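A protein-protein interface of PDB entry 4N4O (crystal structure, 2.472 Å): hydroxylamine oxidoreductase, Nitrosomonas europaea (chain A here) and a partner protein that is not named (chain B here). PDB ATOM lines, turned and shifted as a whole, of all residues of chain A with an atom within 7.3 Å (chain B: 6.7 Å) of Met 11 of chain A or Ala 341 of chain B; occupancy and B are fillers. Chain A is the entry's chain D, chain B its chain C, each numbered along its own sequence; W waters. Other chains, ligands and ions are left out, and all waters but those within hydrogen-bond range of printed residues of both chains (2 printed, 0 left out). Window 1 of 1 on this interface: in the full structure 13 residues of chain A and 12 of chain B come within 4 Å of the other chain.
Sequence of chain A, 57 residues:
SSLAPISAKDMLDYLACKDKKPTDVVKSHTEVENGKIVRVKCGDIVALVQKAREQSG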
ATOM      1  N   LEU A   3      -3.139   6.002 -14.638  1.00  0.00           N
ATOM      2  CA  LEU A   3      -2.288   6.100 -15.830  1.00  0.00           C
ATOM      3  C   LEU A   3      -1.033   6.947 -15.627  1.00  0.00           C
ATOM      4  O   LEU A   3      -1.071   7.985 -14.961  1.00  0.00           O
ATOM      5  CB  LEU A   3      -3.093   6.645 -17.017  1.00  0.00           C
ATOM      6  CG  LEU A   3      -3.319   5.787 -18.271  1.00  0.00           C
ATOM      7  CD1 LEU A   3      -3.545   4.305 -17.971  1.00  0.00           C
ATOM      8  CD2 LEU A   3      -4.470   6.356 -19.102  1.00  0.00           C
ATOM      9  N   ILE A   6       1.771  11.228 -19.811  1.00  0.00           N
ATOM     10  CA  ILE A   6       2.374  11.370 -21.136  1.00  0.00           C
ATOM     11  C   ILE A   6       1.945  12.712 -21.722  1.00  0.00           C
ATOM     12  O   ILE A   6       0.749  13.020 -21.774  1.00  0.00           O
ATOM     13  CB  ILE A   6       1.964  10.216 -22.098  1.00  0.00           C
ATOM     14  CG1 ILE A   6       2.387   8.854 -21.535  1.00  0.00           C
ATOM     15  CG2 ILE A   6       2.572  10.426 -23.491  1.00  0.00           C
ATOM     16  CD1 ILE A   6       1.655   7.672 -22.147  1.00  0.00           C
ATOM     17  N   SER A   7       2.925  13.505 -22.152  1.00  0.00           N
ATOM     18  CA  SER A   7       2.667  14.825 -22.725  1.00  0.00           C
ATOM     19  C   SER A   7       1.886  14.733 -24.036  1.00  0.00           C
ATOM     20  O   SER A   7       1.937  13.716 -24.733  1.00  0.00           O
ATOM     21  CB  SER A   7       3.980  15.584 -22.934  1.00  0.00           C
ATOM     22  OG  SER A   7       4.777  14.960 -23.926  1.00  0.00           O
ATOM     23  N   ALA A   8       1.165  15.805 -24.360  1.00  0.00           N
ATOM     24  CA  ALA A   8       0.328  15.859 -25.559  1.00  0.00           C
ATOM     25  C   ALA A   8       1.123  15.714 -26.857  1.00  0.00           C
ATOM     26  O   ALA A   8       0.649  15.083 -27.804  1.00  0.00           O
ATOM     27  CB  ALA A   8      -0.489  17.134 -25.575  1.00  0.00           C
ATOM     28  N   LYS A   9       2.324  16.295 -26.897  1.00  0.00           N
ATOM     29  CA  LYS A   9       3.205  16.174 -28.062  1.00  0.00           C
ATOM     30  C   LYS A   9       3.587  14.719 -28.321  1.00  0.00           C
ATOM     31  O   LYS A   9       3.594  14.268 -29.466  1.00  0.00           O
ATOM     32  CB  LYS A   9       4.461  17.051 -27.923  1.00  0.00           C
ATOM     33  CG  LYS A   9       5.338  16.772 -26.701  1.00  0.00           C
ATOM     34  CD  LYS A   9       6.638  17.566 -26.748  1.00  0.00           C
ATOM     35  CE  LYS A   9       7.758  16.790 -27.432  1.00  0.00           C
ATOM     36  NZ  LYS A   9       8.323  15.738 -26.536  1.00  0.00           N
ATOM     37  N   ASP A  10       3.886  13.993 -27.245  1.00  0.00           N
ATOM     38  CA  ASP A  10       4.209  12.576 -27.326  1.00  0.00           C
ATOM     39  C   ASP A  10       2.987  11.744 -27.707  1.00  0.00           C
ATOM     40  O   ASP A  10       3.118  10.708 -28.359  1.00  0.00           O
ATOM     41  CB  ASP A  10       4.817  12.087 -26.007  1.00  0.00           C
ATOM     42  CG  ASP A  10       6.225  12.616 -25.782  1.00  0.00           C
ATOM     43  OD1 ASP A  10       6.574  12.902 -24.618  1.00  0.00           O
ATOM     44  OD2 ASP A  10       6.985  12.747 -26.766  1.00  0.00           O
ATOM     45  N   MET A  11       1.806  12.207 -27.305  1.00  0.00           N
ATOM     46  CA  MET A  11       0.549  11.593 -27.729  1.00  0.00           C
ATOM     47  C   MET A  11       0.289  11.825 -29.218  1.00  0.00           C
ATOM     48  O   MET A  11      -0.147  10.911 -29.920  1.00  0.00           O
ATOM     49  CB  MET A  11      -0.625  12.100 -26.885  1.00  0.00           C
ATOM     50  CG  MET A  11      -0.659  11.568 -25.450  1.00  0.00           C
ATOM     51  SD  MET A  11      -0.713   9.764 -25.311  1.00  0.00           S
ATOM     52  CE  MET A  11      -2.214   9.366 -26.211  1.00  0.00           C
ATOM     53  N   LEU A  12       0.566  13.042 -29.692  1.00  0.00           N
ATOM     54  CA  LEU A  12       0.439  13.374 -31.115  1.00  0.00           C
ATOM     55  C   LEU A  12       1.386  12.549 -31.981  1.00  0.00           C
ATOM     56  O   LEU A  12       0.962  11.945 -32.970  1.00  0.00           O
ATOM     57  CB  LEU A  12       0.686  14.866 -31.375  1.00  0.00           C
ATOM     58  CG  LEU A  12      -0.455  15.887 -31.494  1.00  0.00           C
ATOM     59  CD1 LEU A  12      -1.807  15.246 -31.795  1.00  0.00           C
ATOM     60  CD2 LEU A  12      -0.536  16.773 -30.265  1.00  0.00           C
ATOM     61  N   ASP A  13       2.664  12.530 -31.600  1.00  0.00           N
ATOM     62  CA  ASP A  13       3.696  11.798 -32.338  1.00  0.00           C
ATOM     63  C   ASP A  13       3.409  10.302 -32.381  1.00  0.00           C
ATOM     64  O   ASP A  13       3.684   9.644 -33.382  1.00  0.00           O
ATOM     65  CB  ASP A  13       5.082  12.058 -31.739  1.00  0.00           C
ATOM     66  CG  ASP A  13       5.481  13.523 -31.792  1.00  0.00           C
ATOM     67  OD1 ASP A  13       5.060  14.233 -32.731  1.00  0.00           O
ATOM     68  OD2 ASP A  13       6.222  13.963 -30.890  1.00  0.00           O
ATOM     69  N   TYR A  14       2.847   9.778 -31.292  1.00  0.00           N
ATOM     70  CA  TYR A  14       2.436   8.380 -31.223  1.00  0.00           C
ATOM     71  C   TYR A  14       1.309   8.082 -32.211  1.00  0.00           C
ATOM     72  O   TYR A  14       1.372   7.095 -32.947  1.00  0.00           O
ATOM     73  CB  TYR A  14       2.019   8.014 -29.794  1.00  0.00           C
ATOM     74  CG  TYR A  14       1.544   6.589 -29.626  1.00  0.00           C
ATOM     75  CD1 TYR A  14       2.447   5.525 -29.629  1.00  0.00           C
ATOM     76  CD2 TYR A  14       0.188   6.305 -29.457  1.00  0.00           C
ATOM     77  CE1 TYR A  14       2.011   4.211 -29.473  1.00  0.00           C
ATOM     78  CE2 TYR A  14      -0.258   4.997 -29.300  1.00  0.00           C
ATOM     79  CZ  TYR A  14       0.658   3.955 -29.309  1.00  0.00           C
ATOM     80  OH  TYR A  14       0.219   2.662 -29.154  1.00  0.00           O
ATOM     81  N   LEU A  15       0.293   8.944 -32.228  1.00  0.00           N
ATOM     82  CA  LEU A  15      -0.841   8.805 -33.142  1.00  0.00           C
ATOM     83  C   LEU A  15      -0.446   9.012 -34.602  1.00  0.00           C
ATOM     84  O   LEU A  15      -1.015   8.380 -35.493  1.00  0.00           O
ATOM     85  CB  LEU A  15      -1.968   9.768 -32.761  1.00  0.00           C
ATOM     86  CG  LEU A  15      -2.873   9.383 -31.587  1.00  0.00           C
ATOM     87  CD1 LEU A  15      -3.617  10.604 -31.078  1.00  0.00           C
ATOM     88  CD2 LEU A  15      -3.854   8.277 -31.975  1.00  0.00           C
ATOM     89  N   ALA A  16       0.527   9.893 -34.837  1.00  0.00           N
ATOM     90  CA  ALA A  16       1.043  10.152 -36.183  1.00  0.00           C
ATOM     91  C   ALA A  16       1.708   8.914 -36.771  1.00  0.00           C
ATOM     92  O   ALA A  16       1.781   8.755 -37.990  1.00  0.00           O
ATOM     93  CB  ALA A  16       2.023  11.315 -36.162  1.00  0.00           C
ATOM     94  N   CYS A  17       2.178   8.039 -35.888  1.00  0.00           N
ATOM     95  CA  CYS A  17       2.897   6.833 -36.281  1.00  0.00           C
ATOM     96  C   CYS A  17       2.006   5.596 -36.400  1.00  0.00           C
ATOM     97  O   CYS A  17       2.505   4.474 -36.515  1.00  0.00           O
ATOM     98  CB  CYS A  17       4.050   6.586 -35.311  1.00  0.00           C
ATOM     99  SG  CYS A  17       5.407   7.740 -35.558  1.00  0.00           S
ATOM    100  N   ILE A  45       9.208   7.054 -30.521  1.00  0.00           N
ATOM    101  CA  ILE A  45       7.978   7.476 -29.848  1.00  0.00           C
ATOM    102  C   ILE A  45       7.133   6.290 -29.363  1.00  0.00           C
ATOM    103  O   ILE A  45       6.532   6.353 -28.287  1.00  0.00           O
ATOM    104  CB  ILE A  45       7.140   8.492 -30.698  1.00  0.00           C
ATOM    105  CG1 ILE A  45       5.963   9.051 -29.888  1.00  0.00           C
ATOM    106  CG2 ILE A  45       6.655   7.878 -32.007  1.00  0.00           C
ATOM    107  CD1 ILE A  45       6.372   9.826 -28.651  1.00  0.00           C
ATOM    108  N   LEU A  48       8.893   5.157 -26.384  1.00  0.00           N
ATOM    109  CA  LEU A  48       8.654   6.135 -25.319  1.00  0.00           C
ATOM    110  C   LEU A  48       7.305   5.899 -24.634  1.00  0.00           C
ATOM    111  O   LEU A  48       7.196   6.012 -23.410  1.00  0.00           O
ATOM    112  CB  LEU A  48       8.728   7.562 -25.889  1.00  0.00           C
ATOM    113  CG  LEU A  48       8.908   8.824 -25.023  1.00  0.00           C
ATOM    114  CD1 LEU A  48       7.616   9.254 -24.319  1.00  0.00           C
ATOM    115  CD2 LEU A  48      10.065   8.695 -24.025  1.00  0.00           C
ATOM    116  N   VAL A  49       6.290   5.572 -25.431  1.00  0.00           N
ATOM    117  CA  VAL A  49       4.945   5.305 -24.921  1.00  0.00           C
ATOM    118  C   VAL A  49       4.871   3.937 -24.233  1.00  0.00           C
ATOM    119  O   VAL A  49       4.346   3.831 -23.123  1.00  0.00           O
ATOM    120  CB  VAL A  49       3.863   5.444 -26.033  1.00  0.00           C
ATOM    121  CG1 VAL A  49       2.497   4.969 -25.545  1.00  0.00           C
ATOM    122  CG2 VAL A  49       3.773   6.886 -26.507  1.00  0.00           C
ATOM    123  N   ARG A  53       3.612   3.182 -20.504  1.00  0.00           N
ATOM    124  CA  ARG A  53       2.494   2.246 -20.324  1.00  0.00           C
ATOM    125  C   ARG A  53       2.848   1.121 -19.351  1.00  0.00           C
ATOM    126  O   ARG A  53       1.964   0.484 -18.774  1.00  0.00           O
ATOM    127  CB  ARG A  53       2.068   1.642 -21.668  1.00  0.00           C
ATOM    128  CG  ARG A  53       1.389   2.608 -22.637  1.00  0.00           C
ATOM    129  CD  ARG A  53      -0.118   2.693 -22.423  1.00  0.00           C
ATOM    130  NE  ARG A  53      -0.793   3.225 -23.607  1.00  0.00           N
ATOM    131  CZ  ARG A  53      -1.083   4.509 -23.806  1.00  0.00           C
ATOM    132  NH1 ARG A  53      -0.770   5.422 -22.897  1.00  0.00           N
ATOM    133  NH2 ARG A  53      -1.694   4.880 -24.921  1.00  0.00           N
ATOM    134  N   GLN B 196     -10.157   9.115 -13.771  1.00  0.00           N
ATOM    135  CA  GLN B 196      -9.931  10.454 -14.323  1.00  0.00           C
ATOM    136  C   GLN B 196     -10.875  11.483 -13.706  1.00  0.00           C
ATOM    137  O   GLN B 196     -10.474  12.606 -13.394  1.00  0.00           O
ATOM    138  CB  GLN B 196     -10.089  10.438 -15.846  1.00  0.00           C
ATOM    139  CG  GLN B 196      -8.885   9.886 -16.611  1.00  0.00           C
ATOM    140  CD  GLN B 196      -8.876   8.368 -16.747  1.00  0.00           C
ATOM    141  OE1 GLN B 196      -9.723   7.668 -16.192  1.00  0.00           O
ATOM    142  NE2 GLN B 196      -7.906   7.855 -17.497  1.00  0.00           N
ATOM    143  N   ARG B 330     -15.603  10.991 -23.819  1.00  0.00           N
ATOM    144  CA  ARG B 330     -14.194  10.598 -23.867  1.00  0.00           C
ATOM    145  C   ARG B 330     -13.282  11.705 -23.341  1.00  0.00           C
ATOM    146  O   ARG B 330     -12.407  11.457 -22.511  1.00  0.00           O
ATOM    147  CB  ARG B 330     -13.775  10.223 -25.290  1.00  0.00           C
ATOM    148  CG  ARG B 330     -14.651   9.184 -25.976  1.00  0.00           C
ATOM    149  CD  ARG B 330     -14.003   8.714 -27.261  1.00  0.00           C
ATOM    150  NE  ARG B 330     -13.709   9.823 -28.162  1.00  0.00           N
ATOM    151  CZ  ARG B 330     -12.661   9.879 -28.979  1.00  0.00           C
ATOM    152  NH1 ARG B 330     -11.775   8.890 -29.024  1.00  0.00           N
ATOM    153  NH2 ARG B 330     -12.497  10.939 -29.754  1.00  0.00           N
ATOM    154  N   TRP B 331     -13.492  12.922 -23.835  1.00  0.00           N
ATOM    155  CA  TRP B 331     -12.680  14.070 -23.444  1.00  0.00           C
ATOM    156  C   TRP B 331     -13.184  14.755 -22.177  1.00  0.00           C
ATOM    157  O   TRP B 331     -12.386  15.233 -21.369  1.00  0.00           O
ATOM    158  CB  TRP B 331     -12.604  15.083 -24.583  1.00  0.00           C
ATOM    159  CG  TRP B 331     -11.596  14.739 -25.636  1.00  0.00           C
ATOM    160  CD1 TRP B 331     -11.851  14.292 -26.900  1.00  0.00           C
ATOM    161  CD2 TRP B 331     -10.169  14.820 -25.519  1.00  0.00           C
ATOM    162  NE1 TRP B 331     -10.675  14.090 -27.577  1.00  0.00           N
ATOM    163  CE2 TRP B 331      -9.626  14.405 -26.754  1.00  0.00           C
ATOM    164  CE3 TRP B 331      -9.298  15.204 -24.490  1.00  0.00           C
ATOM    165  CZ2 TRP B 331      -8.247  14.361 -26.991  1.00  0.00           C
ATOM    166  CZ3 TRP B 331      -7.925  15.158 -24.724  1.00  0.00           C
ATOM    167  CH2 TRP B 331      -7.416  14.741 -25.967  1.00  0.00           C
ATOM    168  N   PRO B 335      -9.605  19.081 -21.395  1.00  0.00           N
ATOM    169  CA  PRO B 335      -8.599  18.162 -21.930  1.00  0.00           C
ATOM    170  C   PRO B 335      -7.342  18.039 -21.065  1.00  0.00           C
ATOM    171  O   PRO B 335      -6.530  17.135 -21.282  1.00  0.00           O
ATOM    172  CB  PRO B 335      -8.241  18.786 -23.288  1.00  0.00           C
ATOM    173  CG  PRO B 335      -9.264  19.864 -23.527  1.00  0.00           C
ATOM    174  CD  PRO B 335      -9.651  20.328 -22.175  1.00  0.00           C
ATOM    175  N   PHE B 336      -7.197  18.938 -20.093  1.00  0.00           N
ATOM    176  CA  PHE B 336      -6.007  19.018 -19.247  1.00  0.00           C
ATOM    177  C   PHE B 336      -6.100  18.153 -17.987  1.00  0.00           C
ATOM    178  O   PHE B 336      -5.142  18.066 -17.215  1.00  0.00           O
ATOM    179  CB  PHE B 336      -5.741  20.478 -18.860  1.00  0.00           C
ATOM    180  CG  PHE B 336      -6.900  21.141 -18.164  1.00  0.00           C
ATOM    181  CD1 PHE B 336      -7.032  21.074 -16.779  1.00  0.00           C
ATOM    182  CD2 PHE B 336      -7.864  21.830 -18.895  1.00  0.00           C
ATOM    183  CE1 PHE B 336      -8.106  21.682 -16.132  1.00  0.00           C
ATOM    184  CE2 PHE B 336      -8.941  22.440 -18.256  1.00  0.00           C
ATOM    185  CZ  PHE B 336      -9.062  22.368 -16.874  1.00  0.00           C
ATOM    186  N   VAL B 337      -7.259  17.534 -17.774  1.00  0.00           N
ATOM    187  CA  VAL B 337      -7.482  16.679 -16.609  1.00  0.00           C
ATOM    188  C   VAL B 337      -6.592  15.437 -16.718  1.00  0.00           C
ATOM    189  O   VAL B 337      -6.620  14.750 -17.739  1.00  0.00           O
ATOM    190  CB  VAL B 337      -8.986  16.304 -16.450  1.00  0.00           C
ATOM    191  CG1 VAL B 337      -9.186  15.215 -15.397  1.00  0.00           C
ATOM    192  CG2 VAL B 337      -9.807  17.534 -16.091  1.00  0.00           C
ATOM    193  N   PRO B 338      -5.776  15.167 -15.677  1.00  0.00           N
ATOM    194  CA  PRO B 338      -4.836  14.041 -15.695  1.00  0.00           C
ATOM    195  C   PRO B 338      -5.485  12.719 -16.114  1.00  0.00           C
ATOM    196  O   PRO B 338      -6.564  12.371 -15.629  1.00  0.00           O
ATOM    197  CB  PRO B 338      -4.354  13.969 -14.243  1.00  0.00           C
ATOM    198  CG  PRO B 338      -4.448  15.373 -13.760  1.00  0.00           C
ATOM    199  CD  PRO B 338      -5.671  15.944 -14.425  1.00  0.00           C
ATOM    200  N   GLY B 339      -4.831  12.009 -17.030  1.00  0.00           N
ATOM    201  CA  GLY B 339      -5.312  10.713 -17.501  1.00  0.00           C
ATOM    202  C   GLY B 339      -6.210  10.761 -18.726  1.00  0.00           C
ATOM    203  O   GLY B 339      -6.321   9.769 -19.448  1.00  0.00           O
ATOM    204  N   ILE B 340      -6.850  11.908 -18.959  1.00  0.00           N
ATOM    205  CA  ILE B 340      -7.813  12.065 -20.058  1.00  0.00           C
ATOM    206  C   ILE B 340      -7.163  11.926 -21.435  1.00  0.00           C
ATOM    207  O   ILE B 340      -7.624  11.137 -22.262  1.00  0.00           O
ATOM    208  CB  ILE B 340      -8.601  13.402 -19.946  1.00  0.00           C
ATOM    209  CG1 ILE B 340      -9.543  13.374 -18.733  1.00  0.00           C
ATOM    210  CG2 ILE B 340      -9.366  13.715 -21.236  1.00  0.00           C
ATOM    211  CD1 ILE B 340     -10.713  12.401 -18.838  1.00  0.00           C
ATOM    212  N   ALA B 341      -6.094  12.689 -21.663  1.00  0.00           N
ATOM    213  CA  ALA B 341      -5.360  12.653 -22.930  1.00  0.00           C
ATOM    214  C   ALA B 341      -4.648  11.318 -23.138  1.00  0.00           C
ATOM    215  O   ALA B 341      -4.567  10.818 -24.260  1.00  0.00           O
ATOM    216  CB  ALA B 341      -4.369  13.797 -22.997  1.00  0.00           C
ATOM    217  N   GLU B 342      -4.142  10.746 -22.050  1.00  0.00           N
ATOM    218  CA  GLU B 342      -3.464   9.449 -22.088  1.00  0.00           C
ATOM    219  C   GLU B 342      -4.447   8.310 -22.390  1.00  0.00           C
ATOM    220  O   GLU B 342      -4.060   7.273 -22.928  1.00  0.00           O
ATOM    221  CB  GLU B 342      -2.731   9.191 -20.766  1.00  0.00           C
ATOM    222  CG  GLU B 342      -1.534  10.110 -20.500  1.00  0.00           C
ATOM    223  CD  GLU B 342      -1.896  11.418 -19.794  1.00  0.00           C
ATOM    224  OE1 GLU B 342      -3.086  11.800 -19.773  1.00  0.00           O
ATOM    225  OE2 GLU B 342      -0.974  12.073 -19.257  1.00  0.00           O
ATOM    226  N   ASN B 343      -5.715   8.530 -22.052  1.00  0.00           N
ATOM    227  CA  ASN B 343      -6.773   7.537 -22.217  1.00  0.00           C
ATOM    228  C   ASN B 343      -7.396   7.525 -23.620  1.00  0.00           C
ATOM    229  O   ASN B 343      -8.067   6.562 -23.998  1.00  0.00           O
ATOM    230  CB  ASN B 343      -7.855   7.761 -21.149  1.00  0.00           C
ATOM    231  CG  ASN B 343      -8.993   6.761 -21.233  1.00  0.00           C
ATOM    232  OD1 ASN B 343      -8.774   5.550 -21.266  1.00  0.00           O
ATOM    233  ND2 ASN B 343     -10.221   7.268 -21.259  1.00  0.00           N
ATOM    234  N   ILE B 344      -7.149   8.581 -24.394  1.00  0.00           N
ATOM    235  CA  ILE B 344      -7.806   8.773 -25.694  1.00  0.00           C
ATOM    236  C   ILE B 344      -7.549   7.648 -26.716  1.00  0.00           C
ATOM    237  O   ILE B 344      -8.290   7.507 -27.692  1.00  0.00           O
ATOM    238  CB  ILE B 344      -7.501  10.184 -26.290  1.00  0.00           C
ATOM    239  CG1 ILE B 344      -8.697  10.707 -27.093  1.00  0.00           C
ATOM    240  CG2 ILE B 344      -6.206  10.189 -27.110  1.00  0.00           C
ATOM    241  CD1 ILE B 344      -9.953  10.941 -26.260  1.00  0.00           C
ATOM    242  N   THR B 345      -6.511   6.849 -26.472  1.00  0.00           N
ATOM    243  CA  THR B 345      -6.123   5.763 -27.376  1.00  0.00           C
ATOM    244  C   THR B 345      -6.608   4.384 -26.914  1.00  0.00           C
ATOM    245  O   THR B 345      -6.524   3.412 -27.667  1.00  0.00           O
ATOM    246  CB  THR B 345      -4.591   5.714 -27.574  1.00  0.00           C
ATOM    247  OG1 THR B 345      -3.938   5.805 -26.300  1.00  0.00           O
ATOM    248  CG2 THR B 345      -4.127   6.860 -28.459  1.00  0.00           C
ATOM    249  N   LEU B 381      -5.381  17.734 -28.591  1.00  0.00           N
ATOM    250  CA  LEU B 381      -4.032  17.448 -28.101  1.00  0.00           C
ATOM    251  C   LEU B 381      -3.027  18.528 -28.501  1.00  0.00           C
ATOM    252  O   LEU B 381      -2.082  18.804 -27.765  1.00  0.00           O
ATOM    253  CB  LEU B 381      -3.556  16.076 -28.592  1.00  0.00           C
ATOM    254  CG  LEU B 381      -4.232  14.810 -28.055  1.00  0.00           C
ATOM    255  CD1 LEU B 381      -3.913  13.629 -28.954  1.00  0.00           C
ATOM    256  CD2 LEU B 381      -3.816  14.517 -26.622  1.00  0.00           C
ATOM    257  N   LEU B 384      -3.668  21.260 -26.018  1.00  0.00           N
ATOM    258  CA  LEU B 384      -3.117  20.819 -24.737  1.00  0.00           C
ATOM    259  C   LEU B 384      -1.603  21.025 -24.643  1.00  0.00           C
ATOM    260  O   LEU B 384      -1.108  21.527 -23.634  1.00  0.00           O
ATOM    261  CB  LEU B 384      -3.477  19.351 -24.477  1.00  0.00           C
ATOM    262  CG  LEU B 384      -2.980  18.694 -23.183  1.00  0.00           C
ATOM    263  CD1 LEU B 384      -3.486  19.413 -21.943  1.00  0.00           C
ATOM    264  CD2 LEU B 384      -3.389  17.237 -23.147  1.00  0.00           C
ATOM    265  N   GLN B 388       0.581  23.080 -22.052  1.00  0.00           N
ATOM    266  CA  GLN B 388       1.564  22.343 -21.255  1.00  0.00           C
ATOM    267  C   GLN B 388       2.952  22.979 -21.280  1.00  0.00           C
ATOM    268  O   GLN B 388       3.661  22.963 -20.272  1.00  0.00           O
ATOM    269  CB  GLN B 388       1.626  20.871 -21.683  1.00  0.00           C
ATOM    270  CG  GLN B 388       0.474  20.024 -21.138  1.00  0.00           C
ATOM    271  CD  GLN B 388       0.513  18.569 -21.585  1.00  0.00           C
ATOM    272  OE1 GLN B 388       1.345  18.167 -22.401  1.00  0.00           O
ATOM    273  NE2 GLN B 388      -0.399  17.770 -21.047  1.00  0.00           N
HETATM  274  O   HOH W   1       2.714  18.272 -24.666  1.00  0.00           O
HETATM  275  O   HOH W   2      -0.970  15.086 -21.532  1.00  0.00           O
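The side-chain hydroxyl of Thr 345 of chain B sits at hydrogen-bond distance from the guanidinium group of Arg 53 of chain A (2.8 Å). OE1 of Gln 388 of chain B sits at hydrogen-bond distance from N of Ala 8 of chain A, 3.1 Å away. OE2 of Glu 342 of chain B lies within hydrogen-bond range of N of Ile 6 of chain A.
Printed residues of chain B within 4 Å of Met 11 of chain A: Ala 341 and Thr 345. Ala 341 of chain B touches one residue of chain A. Of the printed residues of chain A, Gly 339 of chain B touches Leu 3 (3.9 Å). Of the printed residues of chain B, Ala 8 of chain A touches Leu 381, Leu 384 and Gln 388. Printed residues of chain A within 4 Å of Gln 388 of chain B: Ser 7 (3.6 Å) and Ala 8 (3.1 Å). Asp 13 of chain A touches none of the printed residues of chain B. The nearest residue of chain A that does not touch Ala 341 of chain B is Ile 6 of chain A (5.3 Å).
Printed residues of chain B that touch a printed residue of chain A: Gly 339, Ala 341, Glu 342, Asn 343, Thr 345, Leu 381, Leu 384 and Gln 388. Hydrophobic or aromatic side chains of chain B that line the printed part of chain A: Leu 381 and Leu 384. Along chain B the printed residues that touch a printed residue of chain A span positions 339 to 388. Of the 17 printed residues of chain A, 8 touch a printed residue of chain B. Along chain A the printed residues that touch a printed residue of chain B span positions 3 to 53. Among the printed residues, 15 pairs touch across the chains. Among the printed residues, no Asp or Glu carboxylate lies within 4 Å of a Lys or Arg side-chain nitrogen of the other chain.
N of Gly 339 of chain B lies within hydrogen-bond range of OE1 of Glu 342 of chain B (3.3 Å). The side-chain hydroxyl (OG) of Ser 7 of chain A lies within hydrogen-bond range of the side-chain carboxylate (OD1) of Asp 10 of chain A. The side-chain amide nitrogen of Gln 196 of chain B sits at hydrogen-bond distance from the backbone carbonyl oxygen of Gly 339 of chain B, at 3.2 Å.
Water W1 lies within hydrogen-bond range of the side-chain amide oxygen of Gln 388 of chain B, the backbone NH of Ala 8 of chain A and the backbone NH of Lys 9 of chain A. Water W2 bridges O of Ile 6 of chain A (2.7 Å) and NE2 of Gln 388 of chain B (2.8 Å).
Gly 339 of chain B touches Leu 3 of chain A (O to CD2, 3.9 Å). CB of Glu 342 of chain B touches CD2 of Leu 3 of chain A, 3.7 Å away. Leu 3 of chain A touches Asn 343 of chain B (CD2 to N, 3.9 Å). O of Leu 381 of chain B touches CB of Ala 8 of chain A, 3.2 Å away. CB of Ala 8 of chain A touches CD2 of Leu 384 of chain B, 3.8 Å away. CE of Met 11 of chain A touches O of Ala 341 of chain B, at 3.4 Å. Thr 345 of chain B touches Met 11 of chain A (CG2 to CE, 3.9 Å). Leu 381 of chain B touches Leu 12 of chain A. Leu 15 of chain A touches Thr 345 of chain B. Arg 53 of chain A touches Glu 342 of chain B (NH1 to O, 3.8 Å).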
